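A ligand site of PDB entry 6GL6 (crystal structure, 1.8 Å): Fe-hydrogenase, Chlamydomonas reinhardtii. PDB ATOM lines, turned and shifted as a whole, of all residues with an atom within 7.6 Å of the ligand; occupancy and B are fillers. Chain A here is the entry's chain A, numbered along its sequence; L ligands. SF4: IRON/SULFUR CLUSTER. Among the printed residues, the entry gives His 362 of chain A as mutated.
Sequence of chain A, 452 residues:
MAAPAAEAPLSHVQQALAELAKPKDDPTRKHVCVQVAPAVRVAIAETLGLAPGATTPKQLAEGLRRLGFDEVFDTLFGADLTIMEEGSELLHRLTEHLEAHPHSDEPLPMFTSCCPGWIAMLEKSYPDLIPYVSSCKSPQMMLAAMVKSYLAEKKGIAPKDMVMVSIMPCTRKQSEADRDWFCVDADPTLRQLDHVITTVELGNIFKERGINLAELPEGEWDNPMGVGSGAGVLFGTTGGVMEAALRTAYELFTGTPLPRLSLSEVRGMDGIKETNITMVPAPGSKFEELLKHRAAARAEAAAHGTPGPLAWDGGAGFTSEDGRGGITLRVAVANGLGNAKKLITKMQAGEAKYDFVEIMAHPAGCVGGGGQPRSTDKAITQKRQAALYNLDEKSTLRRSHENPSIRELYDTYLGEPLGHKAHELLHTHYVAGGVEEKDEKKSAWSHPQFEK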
ATOM      1  N   ALA A  39     -21.804  19.729   6.939  1.00  0.00           N
ATOM      2  CA  ALA A  39     -20.387  20.101   6.931  1.00  0.00           C
ATOM      3  C   ALA A  39     -19.935  20.634   8.294  1.00  0.00           C
ATOM      4  O   ALA A  39     -18.760  20.531   8.654  1.00  0.00           O
ATOM      5  CB  ALA A  39     -20.117  21.142   5.856  1.00  0.00           C
ATOM      6  N   CYS A 114     -27.800  26.665  -4.748  1.00  0.00           N
ATOM      7  CA  CYS A 114     -27.629  26.580  -3.295  1.00  0.00           C
ATOM      8  C   CYS A 114     -26.419  27.363  -2.781  1.00  0.00           C
ATOM      9  O   CYS A 114     -26.399  27.753  -1.619  1.00  0.00           O
ATOM     10  CB  CYS A 114     -27.494  25.124  -2.842  1.00  0.00           C
ATOM     11  SG  CYS A 114     -26.122  24.245  -3.578  1.00  0.00           S
ATOM     12  N   CYS A 115     -25.423  27.585  -3.632  1.00  0.00           N
ATOM     13  CA  CYS A 115     -24.218  28.295  -3.211  1.00  0.00           C
ATOM     14  C   CYS A 115     -24.323  29.799  -3.411  1.00  0.00           C
ATOM     15  O   CYS A 115     -24.388  30.262  -4.551  1.00  0.00           O
ATOM     16  CB  CYS A 115     -23.003  27.795  -3.968  1.00  0.00           C
ATOM     17  SG  CYS A 115     -21.511  28.697  -3.491  1.00  0.00           S
ATOM     18  N   PRO A 116     -24.312  30.580  -2.306  1.00  0.00           N
ATOM     19  CA  PRO A 116     -24.411  32.032  -2.464  1.00  0.00           C
ATOM     20  C   PRO A 116     -23.190  32.679  -3.141  1.00  0.00           C
ATOM     21  O   PRO A 116     -23.314  33.773  -3.707  1.00  0.00           O
ATOM     22  CB  PRO A 116     -24.572  32.544  -1.021  1.00  0.00           C
ATOM     23  CG  PRO A 116     -24.134  31.427  -0.154  1.00  0.00           C
ATOM     24  CD  PRO A 116     -24.343  30.162  -0.897  1.00  0.00           C
ATOM     25  N   GLY A 117     -22.036  32.012  -3.097  1.00  0.00           N
ATOM     26  CA  GLY A 117     -20.869  32.475  -3.821  1.00  0.00           C
ATOM     27  C   GLY A 117     -21.091  32.449  -5.321  1.00  0.00           C
ATOM     28  O   GLY A 117     -20.681  33.362  -6.053  1.00  0.00           O
ATOM     29  N   TRP A 118     -21.738  31.392  -5.793  1.00  0.00           N
ATOM     30  CA  TRP A 118     -22.164  31.293  -7.186  1.00  0.00           C
ATOM     31  C   TRP A 118     -23.210  32.353  -7.498  1.00  0.00           C
ATOM     32  O   TRP A 118     -23.088  33.091  -8.474  1.00  0.00           O
ATOM     33  CB  TRP A 118     -22.701  29.874  -7.459  1.00  0.00           C
ATOM     34  CG  TRP A 118     -23.642  29.728  -8.616  1.00  0.00           C
ATOM     35  CD1 TRP A 118     -24.864  29.103  -8.599  1.00  0.00           C
ATOM     36  CD2 TRP A 118     -23.456  30.195  -9.969  1.00  0.00           C
ATOM     37  NE1 TRP A 118     -25.440  29.170  -9.841  1.00  0.00           N
ATOM     38  CE2 TRP A 118     -24.605  29.826 -10.696  1.00  0.00           C
ATOM     39  CE3 TRP A 118     -22.434  30.900 -10.618  1.00  0.00           C
ATOM     40  CZ2 TRP A 118     -24.757  30.130 -12.059  1.00  0.00           C
ATOM     41  CZ3 TRP A 118     -22.593  31.193 -11.977  1.00  0.00           C
ATOM     42  CH2 TRP A 118     -23.754  30.815 -12.678  1.00  0.00           C
ATOM     43  N   MET A 168     -23.374  27.191   9.781  1.00  0.00           N
ATOM     44  CA  MET A 168     -22.962  26.947   8.405  1.00  0.00           C
ATOM     45  C   MET A 168     -21.447  26.888   8.297  1.00  0.00           C
ATOM     46  O   MET A 168     -20.751  27.388   9.174  1.00  0.00           O
ATOM     47  CB  MET A 168     -23.508  28.051   7.487  1.00  0.00           C
ATOM     48  CG  MET A 168     -25.005  27.982   7.256  1.00  0.00           C
ATOM     49  SD  MET A 168     -25.448  26.564   6.197  1.00  0.00           S
ATOM     50  CE  MET A 168     -27.018  26.074   6.894  1.00  0.00           C
ATOM     51  N   PRO A 169     -20.924  26.261   7.226  1.00  0.00           N
ATOM     52  CA  PRO A 169     -19.478  26.204   7.046  1.00  0.00           C
ATOM     53  C   PRO A 169     -18.897  27.461   6.416  1.00  0.00           C
ATOM     54  O   PRO A 169     -17.690  27.504   6.181  1.00  0.00           O
ATOM     55  CB  PRO A 169     -19.296  25.010   6.102  1.00  0.00           C
ATOM     56  CG  PRO A 169     -20.518  25.065   5.256  1.00  0.00           C
ATOM     57  CD  PRO A 169     -21.631  25.476   6.184  1.00  0.00           C
ATOM     58  N   CYS A 170     -19.729  28.470   6.141  1.00  0.00           N
ATOM     59  CA  CYS A 170     -19.272  29.692   5.471  1.00  0.00           C
ATOM     60  C   CYS A 170     -20.075  30.898   5.961  1.00  0.00           C
ATOM     61  O   CYS A 170     -21.256  30.774   6.293  1.00  0.00           O
ATOM     62  CB  CYS A 170     -19.411  29.566   3.952  1.00  0.00           C
ATOM     63  SG  CYS A 170     -21.134  29.479   3.384  1.00  0.00           S
ATOM     64  N   THR A 171     -19.436  32.062   5.969  1.00  0.00           N
ATOM     65  CA  THR A 171     -20.084  33.278   6.445  1.00  0.00           C
ATOM     66  C   THR A 171     -21.089  33.811   5.437  1.00  0.00           C
ATOM     67  O   THR A 171     -22.062  34.468   5.802  1.00  0.00           O
ATOM     68  CB  THR A 171     -19.057  34.397   6.744  1.00  0.00           C
ATOM     69  OG1 THR A 171     -18.357  34.753   5.556  1.00  0.00           O
ATOM     70  CG2 THR A 171     -18.056  33.949   7.812  1.00  0.00           C
ATOM     71  N   ARG A 172     -20.860  33.523   4.162  1.00  0.00           N
ATOM     72  CA  ARG A 172     -21.633  34.201   3.139  1.00  0.00           C
ATOM     73  C   ARG A 172     -23.047  33.610   3.010  1.00  0.00           C
ATOM     74  O   ARG A 172     -23.865  34.106   2.224  1.00  0.00           O
ATOM     75  CB  ARG A 172     -20.865  34.193   1.804  1.00  0.00           C
ATOM     76  CG  ARG A 172     -21.108  33.073   0.856  1.00  0.00           C
ATOM     77  CD  ARG A 172     -20.147  33.234  -0.333  1.00  0.00           C
ATOM     78  NE  ARG A 172     -18.778  32.894   0.030  1.00  0.00           N
ATOM     79  CZ  ARG A 172     -17.717  33.088  -0.747  1.00  0.00           C
ATOM     80  NH1 ARG A 172     -17.850  33.650  -1.951  1.00  0.00           N
ATOM     81  NH2 ARG A 172     -16.508  32.727  -0.321  1.00  0.00           N
ATOM     82  N   LYS A 173     -23.359  32.611   3.822  1.00  0.00           N
ATOM     83  CA  LYS A 173     -24.752  32.176   3.989  1.00  0.00           C
ATOM     84  C   LYS A 173     -25.565  33.267   4.696  1.00  0.00           C
ATOM     85  O   LYS A 173     -26.783  33.294   4.610  1.00  0.00           O
ATOM     86  CB  LYS A 173     -24.839  30.849   4.776  1.00  0.00           C
ATOM     87  CG  LYS A 173     -24.634  29.619   3.898  1.00  0.00           C
ATOM     88  CD  LYS A 173     -25.858  29.320   3.049  1.00  0.00           C
ATOM     89  CE  LYS A 173     -25.580  28.287   1.971  1.00  0.00           C
ATOM     90  NZ  LYS A 173     -26.795  28.030   1.152  1.00  0.00           N
ATOM     91  N   GLU A 176     -26.849  35.442   1.870  1.00  0.00           N
ATOM     92  CA  GLU A 176     -27.992  34.732   1.316  1.00  0.00           C
ATOM     93  C   GLU A 176     -29.229  35.026   2.167  1.00  0.00           C
ATOM     94  O   GLU A 176     -30.275  35.402   1.644  1.00  0.00           O
ATOM     95  CB  GLU A 176     -27.724  33.220   1.276  1.00  0.00           C
ATOM     96  CG  GLU A 176     -28.883  32.381   0.742  1.00  0.00           C
ATOM     97  CD  GLU A 176     -28.635  30.895   0.950  1.00  0.00           C
ATOM     98  OE1 GLU A 176     -28.032  30.259   0.067  1.00  0.00           O
ATOM     99  OE2 GLU A 176     -29.045  30.371   2.012  1.00  0.00           O
ATOM    100  N   ASN A 335     -16.196  23.079  -9.005  1.00  0.00           N
ATOM    101  CA  ASN A 335     -15.825  23.552  -7.683  1.00  0.00           C
ATOM    102  C   ASN A 335     -14.718  24.582  -7.786  1.00  0.00           C
ATOM    103  O   ASN A 335     -13.672  24.315  -8.379  1.00  0.00           O
ATOM    104  CB  ASN A 335     -15.390  22.400  -6.794  1.00  0.00           C
ATOM    105  CG  ASN A 335     -16.561  21.512  -6.377  1.00  0.00           C
ATOM    106  OD1 ASN A 335     -17.286  21.816  -5.437  1.00  0.00           O
ATOM    107  ND2 ASN A 335     -16.742  20.407  -7.092  1.00  0.00           N
ATOM    108  N   GLY A 336     -14.969  25.765  -7.213  1.00  0.00           N
ATOM    109  CA  GLY A 336     -14.088  26.918  -7.358  1.00  0.00           C
ATOM    110  C   GLY A 336     -14.635  27.875  -8.401  1.00  0.00           C
ATOM    111  O   GLY A 336     -14.922  27.476  -9.529  1.00  0.00           O
ATOM    112  N   LEU A 337     -14.777  29.156  -8.045  1.00  0.00           N
ATOM    113  CA  LEU A 337     -15.402  30.107  -8.954  1.00  0.00           C
ATOM    114  C   LEU A 337     -14.537  30.390 -10.177  1.00  0.00           C
ATOM    115  O   LEU A 337     -15.055  30.570 -11.268  1.00  0.00           O
ATOM    116  CB  LEU A 337     -15.706  31.418  -8.237  1.00  0.00           C
ATOM    117  CG  LEU A 337     -16.811  31.369  -7.172  1.00  0.00           C
ATOM    118  CD1 LEU A 337     -17.075  32.774  -6.645  1.00  0.00           C
ATOM    119  CD2 LEU A 337     -18.103  30.752  -7.700  1.00  0.00           C
ATOM    120  N   ILE A 359     -22.541  24.685  -9.615  1.00  0.00           N
ATOM    121  CA  ILE A 359     -21.370  25.504  -9.331  1.00  0.00           C
ATOM    122  C   ILE A 359     -21.280  25.791  -7.825  1.00  0.00           C
ATOM    123  O   ILE A 359     -22.206  26.348  -7.235  1.00  0.00           O
ATOM    124  CB  ILE A 359     -21.410  26.840 -10.123  1.00  0.00           C
ATOM    125  CG1 ILE A 359     -21.365  26.555 -11.630  1.00  0.00           C
ATOM    126  CG2 ILE A 359     -20.241  27.747  -9.721  1.00  0.00           C
ATOM    127  CD1 ILE A 359     -21.666  27.770 -12.489  1.00  0.00           C
ATOM    128  N   MET A 360     -20.168  25.372  -7.221  1.00  0.00           N
ATOM    129  CA  MET A 360     -19.887  25.643  -5.810  1.00  0.00           C
ATOM    130  C   MET A 360     -18.621  26.493  -5.725  1.00  0.00           C
ATOM    131  O   MET A 360     -17.669  26.276  -6.476  1.00  0.00           O
ATOM    132  CB  MET A 360     -19.700  24.348  -5.012  1.00  0.00           C
ATOM    133  CG  MET A 360     -20.832  23.349  -5.169  1.00  0.00           C
ATOM    134  SD  MET A 360     -22.367  23.928  -4.439  1.00  0.00           S
ATOM    135  CE  MET A 360     -21.950  23.820  -2.711  1.00  0.00           C
ATOM    136  N   ALA A 361     -18.601  27.455  -4.796  1.00  0.00           N
ATOM    137  CA  ALA A 361     -17.528  28.444  -4.745  1.00  0.00           C
ATOM    138  C   ALA A 361     -16.222  27.906  -4.168  1.00  0.00           C
ATOM    139  O   ALA A 361     -15.151  28.382  -4.544  1.00  0.00           O
ATOM    140  CB  ALA A 361     -17.983  29.658  -3.953  1.00  0.00           C
ATOM    141  N   HIS A 362     -16.280  26.932  -3.266  1.00  0.00           N
ATOM    142  CA  HIS A 362     -15.045  26.376  -2.701  1.00  0.00           C
ATOM    143  C   HIS A 362     -14.617  25.080  -3.384  1.00  0.00           C
ATOM    144  O   HIS A 362     -15.445  24.221  -3.687  1.00  0.00           O
ATOM    145  CB  HIS A 362     -15.183  26.154  -1.193  1.00  0.00           C
ATOM    146  CG  HIS A 362     -15.218  27.431  -0.410  1.00  0.00           C
ATOM    147  ND1 HIS A 362     -16.400  28.045  -0.054  1.00  0.00           N
ATOM    148  CD2 HIS A 362     -14.232  28.240   0.031  1.00  0.00           C
ATOM    149  CE1 HIS A 362     -16.141  29.173   0.587  1.00  0.00           C
ATOM    150  NE2 HIS A 362     -14.828  29.304   0.661  1.00  0.00           N
ATOM    151  N   PRO A 363     -13.294  24.943  -3.641  1.00  0.00           N
ATOM    152  CA  PRO A 363     -12.709  23.779  -4.308  1.00  0.00           C
ATOM    153  C   PRO A 363     -13.181  22.404  -3.830  1.00  0.00           C
ATOM    154  O   PRO A 363     -13.392  21.527  -4.674  1.00  0.00           O
ATOM    155  CB  PRO A 363     -11.217  23.964  -4.030  1.00  0.00           C
ATOM    156  CG  PRO A 363     -11.042  25.432  -4.103  1.00  0.00           C
ATOM    157  CD  PRO A 363     -12.283  26.007  -3.457  1.00  0.00           C
ATOM    158  N   ALA A 364     -13.339  22.204  -2.526  1.00  0.00           N
ATOM    159  CA  ALA A 364     -13.763  20.895  -2.007  1.00  0.00           C
ATOM    160  C   ALA A 364     -15.255  20.871  -1.680  1.00  0.00           C
ATOM    161  O   ALA A 364     -15.758  19.927  -1.075  1.00  0.00           O
ATOM    162  CB  ALA A 364     -12.966  20.535  -0.779  1.00  0.00           C
ATOM    163  N   GLY A 365     -15.977  21.908  -2.115  1.00  0.00           N
ATOM    164  CA  GLY A 365     -17.353  22.081  -1.710  1.00  0.00           C
ATOM    165  C   GLY A 365     -17.428  22.526  -0.254  1.00  0.00           C
ATOM    166  O   GLY A 365     -16.454  23.053   0.294  1.00  0.00           O
ATOM    167  N   CYS A 366     -18.578  22.298   0.373  1.00  0.00           N
ATOM    168  CA  CYS A 366     -18.882  22.964   1.637  1.00  0.00           C
ATOM    169  C   CYS A 366     -17.986  22.511   2.796  1.00  0.00           C
ATOM    170  O   CYS A 366     -17.771  23.258   3.735  1.00  0.00           O
ATOM    171  CB  CYS A 366     -20.344  22.743   2.014  1.00  0.00           C
ATOM    172  SG  CYS A 366     -21.527  23.479   0.863  1.00  0.00           S
ATOM    173  N   VAL A 367     -17.443  21.294   2.726  1.00  0.00           N
ATOM    174  CA  VAL A 367     -16.541  20.857   3.780  1.00  0.00           C
ATOM    175  C   VAL A 367     -15.313  21.765   3.822  1.00  0.00           C
ATOM    176  O   VAL A 367     -14.609  21.804   4.836  1.00  0.00           O
ATOM    177  CB  VAL A 367     -16.108  19.390   3.607  1.00  0.00           C
ATOM    178  CG1 VAL A 367     -17.315  18.455   3.802  1.00  0.00           C
ATOM    179  CG2 VAL A 367     -15.462  19.157   2.251  1.00  0.00           C
ATOM    180  N   GLY A 368     -15.074  22.499   2.736  1.00  0.00           N
ATOM    181  CA  GLY A 368     -13.939  23.413   2.652  1.00  0.00           C
ATOM    182  C   GLY A 368     -14.295  24.888   2.826  1.00  0.00           C
ATOM    183  O   GLY A 368     -13.469  25.749   2.529  1.00  0.00           O
ATOM    184  N   GLY A 369     -15.506  25.178   3.290  1.00  0.00           N
ATOM    185  CA  GLY A 369     -15.955  26.543   3.503  1.00  0.00           C
ATOM    186  C   GLY A 369     -15.044  27.416   4.363  1.00  0.00           C
ATOM    187  O   GLY A 369     -14.237  26.923   5.156  1.00  0.00           O
ATOM    188  N   GLY A 370     -15.201  28.729   4.216  1.00  0.00           N
ATOM    189  CA  GLY A 370     -14.318  29.694   4.846  1.00  0.00           C
ATOM    190  C   GLY A 370     -14.577  29.902   6.319  1.00  0.00           C
ATOM    191  O   GLY A 370     -13.825  30.610   6.993  1.00  0.00           O
ATOM    192  N   GLY A 371     -15.647  29.286   6.831  1.00  0.00           N
ATOM    193  CA  GLY A 371     -15.960  29.308   8.256  1.00  0.00           C
ATOM    194  C   GLY A 371     -15.566  28.020   8.949  1.00  0.00           C
ATOM    195  O   GLY A 371     -15.940  27.796  10.099  1.00  0.00           O
ATOM    196  N   GLN A 372     -14.799  27.175   8.257  1.00  0.00           N
ATOM    197  CA  GLN A 372     -14.368  25.898   8.800  1.00  0.00           C
ATOM    198  C   GLN A 372     -13.020  26.053   9.528  1.00  0.00           C
ATOM    199  O   GLN A 372     -12.279  26.992   9.245  1.00  0.00           O
ATOM    200  CB  GLN A 372     -14.235  24.853   7.681  1.00  0.00           C
ATOM    201  CG  GLN A 372     -15.529  24.495   6.988  1.00  0.00           C
ATOM    202  CD  GLN A 372     -16.397  23.560   7.807  1.00  0.00           C
ATOM    203  OE1 GLN A 372     -16.868  23.921   8.892  1.00  0.00           O
ATOM    204  NE2 GLN A 372     -16.584  22.347   7.315  1.00  0.00           N
HETATM  205 FE1  SF4 L   1     -20.806  27.837  -1.380  1.00  0.00          FE
HETATM  206 FE2  SF4 L   1     -18.501  27.457  -0.025  1.00  0.00          FE
HETATM  207 FE3  SF4 L   1     -20.737  28.277   1.319  1.00  0.00          FE
HETATM  208 FE4  SF4 L   1     -20.598  25.719   0.311  1.00  0.00          FE
HETATM  209  S1  SF4 L   1     -19.261  26.606   1.960  1.00  0.00           S
HETATM  210  S2  SF4 L   1     -22.375  27.166   0.127  1.00  0.00           S
HETATM  211  S3  SF4 L   1     -19.384  26.065  -1.606  1.00  0.00           S
HETATM  212  S4  SF4 L   1     -19.590  29.455  -0.289  1.00  0.00           S
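An iron atom (FE1) of the ligand is bound by the side-chain sulfur of Cys 115 (2.4 Å). The backbone NH of His 362 sits close to a sulfur (S3) of the ligand (3.6 Å). FE2 of the ligand is bound by ND1 of His 362, at 2.2 Å. N of Ala 361 lies close to S3 of the ligand (3.6 Å). S4 of the ligand lies close to NE of Arg 172 (3.5 Å). FE4 of the ligand is bound by SG of Cys 366, at 2.5 Å. The side-chain sulfur of Cys 170 is bound to an iron atom (FE3) of the ligand.
CD of Pro 116 touches S2 of the ligand (3.7 Å). Pro 169 touches the ligand. CE of Lys 173 touches S2 of the ligand, 3.9 Å away. Met 360 touches the ligand (CE to S3, 3.6 Å). CA of Gly 369 touches S1 of the ligand (3.6 Å). Hydrophobic or aromatic side chains that line the ligand: Pro 116, Pro 169, Met 360 and His 362. Within 4 Å of the ligand: Cys 115, Pro 116, Pro 169, Cys 170, Arg 172, Lys 173, Met 360, Ala 361, His 362, Cys 366 and Gly 369. Along chain A the residues within 4 Å of the ligand span positions 115 to 369.
The backbone NH of Gly 117 lies close to the side-chain sulfur of Cys 115 (3.4 Å). The backbone carbonyl oxygen (O) of Pro 169 is in hydrogen-bond range of the backbone NH (N) of Gly 370, 3.4 Å away. The side-chain sulfur (SG) of Cys 115 lies close to the backbone NH (N) of Ala 361, 3.4 Å away. NZ of Lys 173 is in salt-bridge range of OE1 of Glu 176 (2.8 Å). The backbone carbonyl oxygen (O) of Cys 114 lies within hydrogen-bond range of the side-chain amino group (NZ) of Lys 173 (2.8 Å). The side-chain sulfur of Cys 115 lies close to the backbone NH of Trp 118 (3.6 Å). O of Met 360 is in hydrogen-bond range of N of Gly 336 (2.8 Å). O of Pro 169 is in hydrogen-bond range of N of Gly 371.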
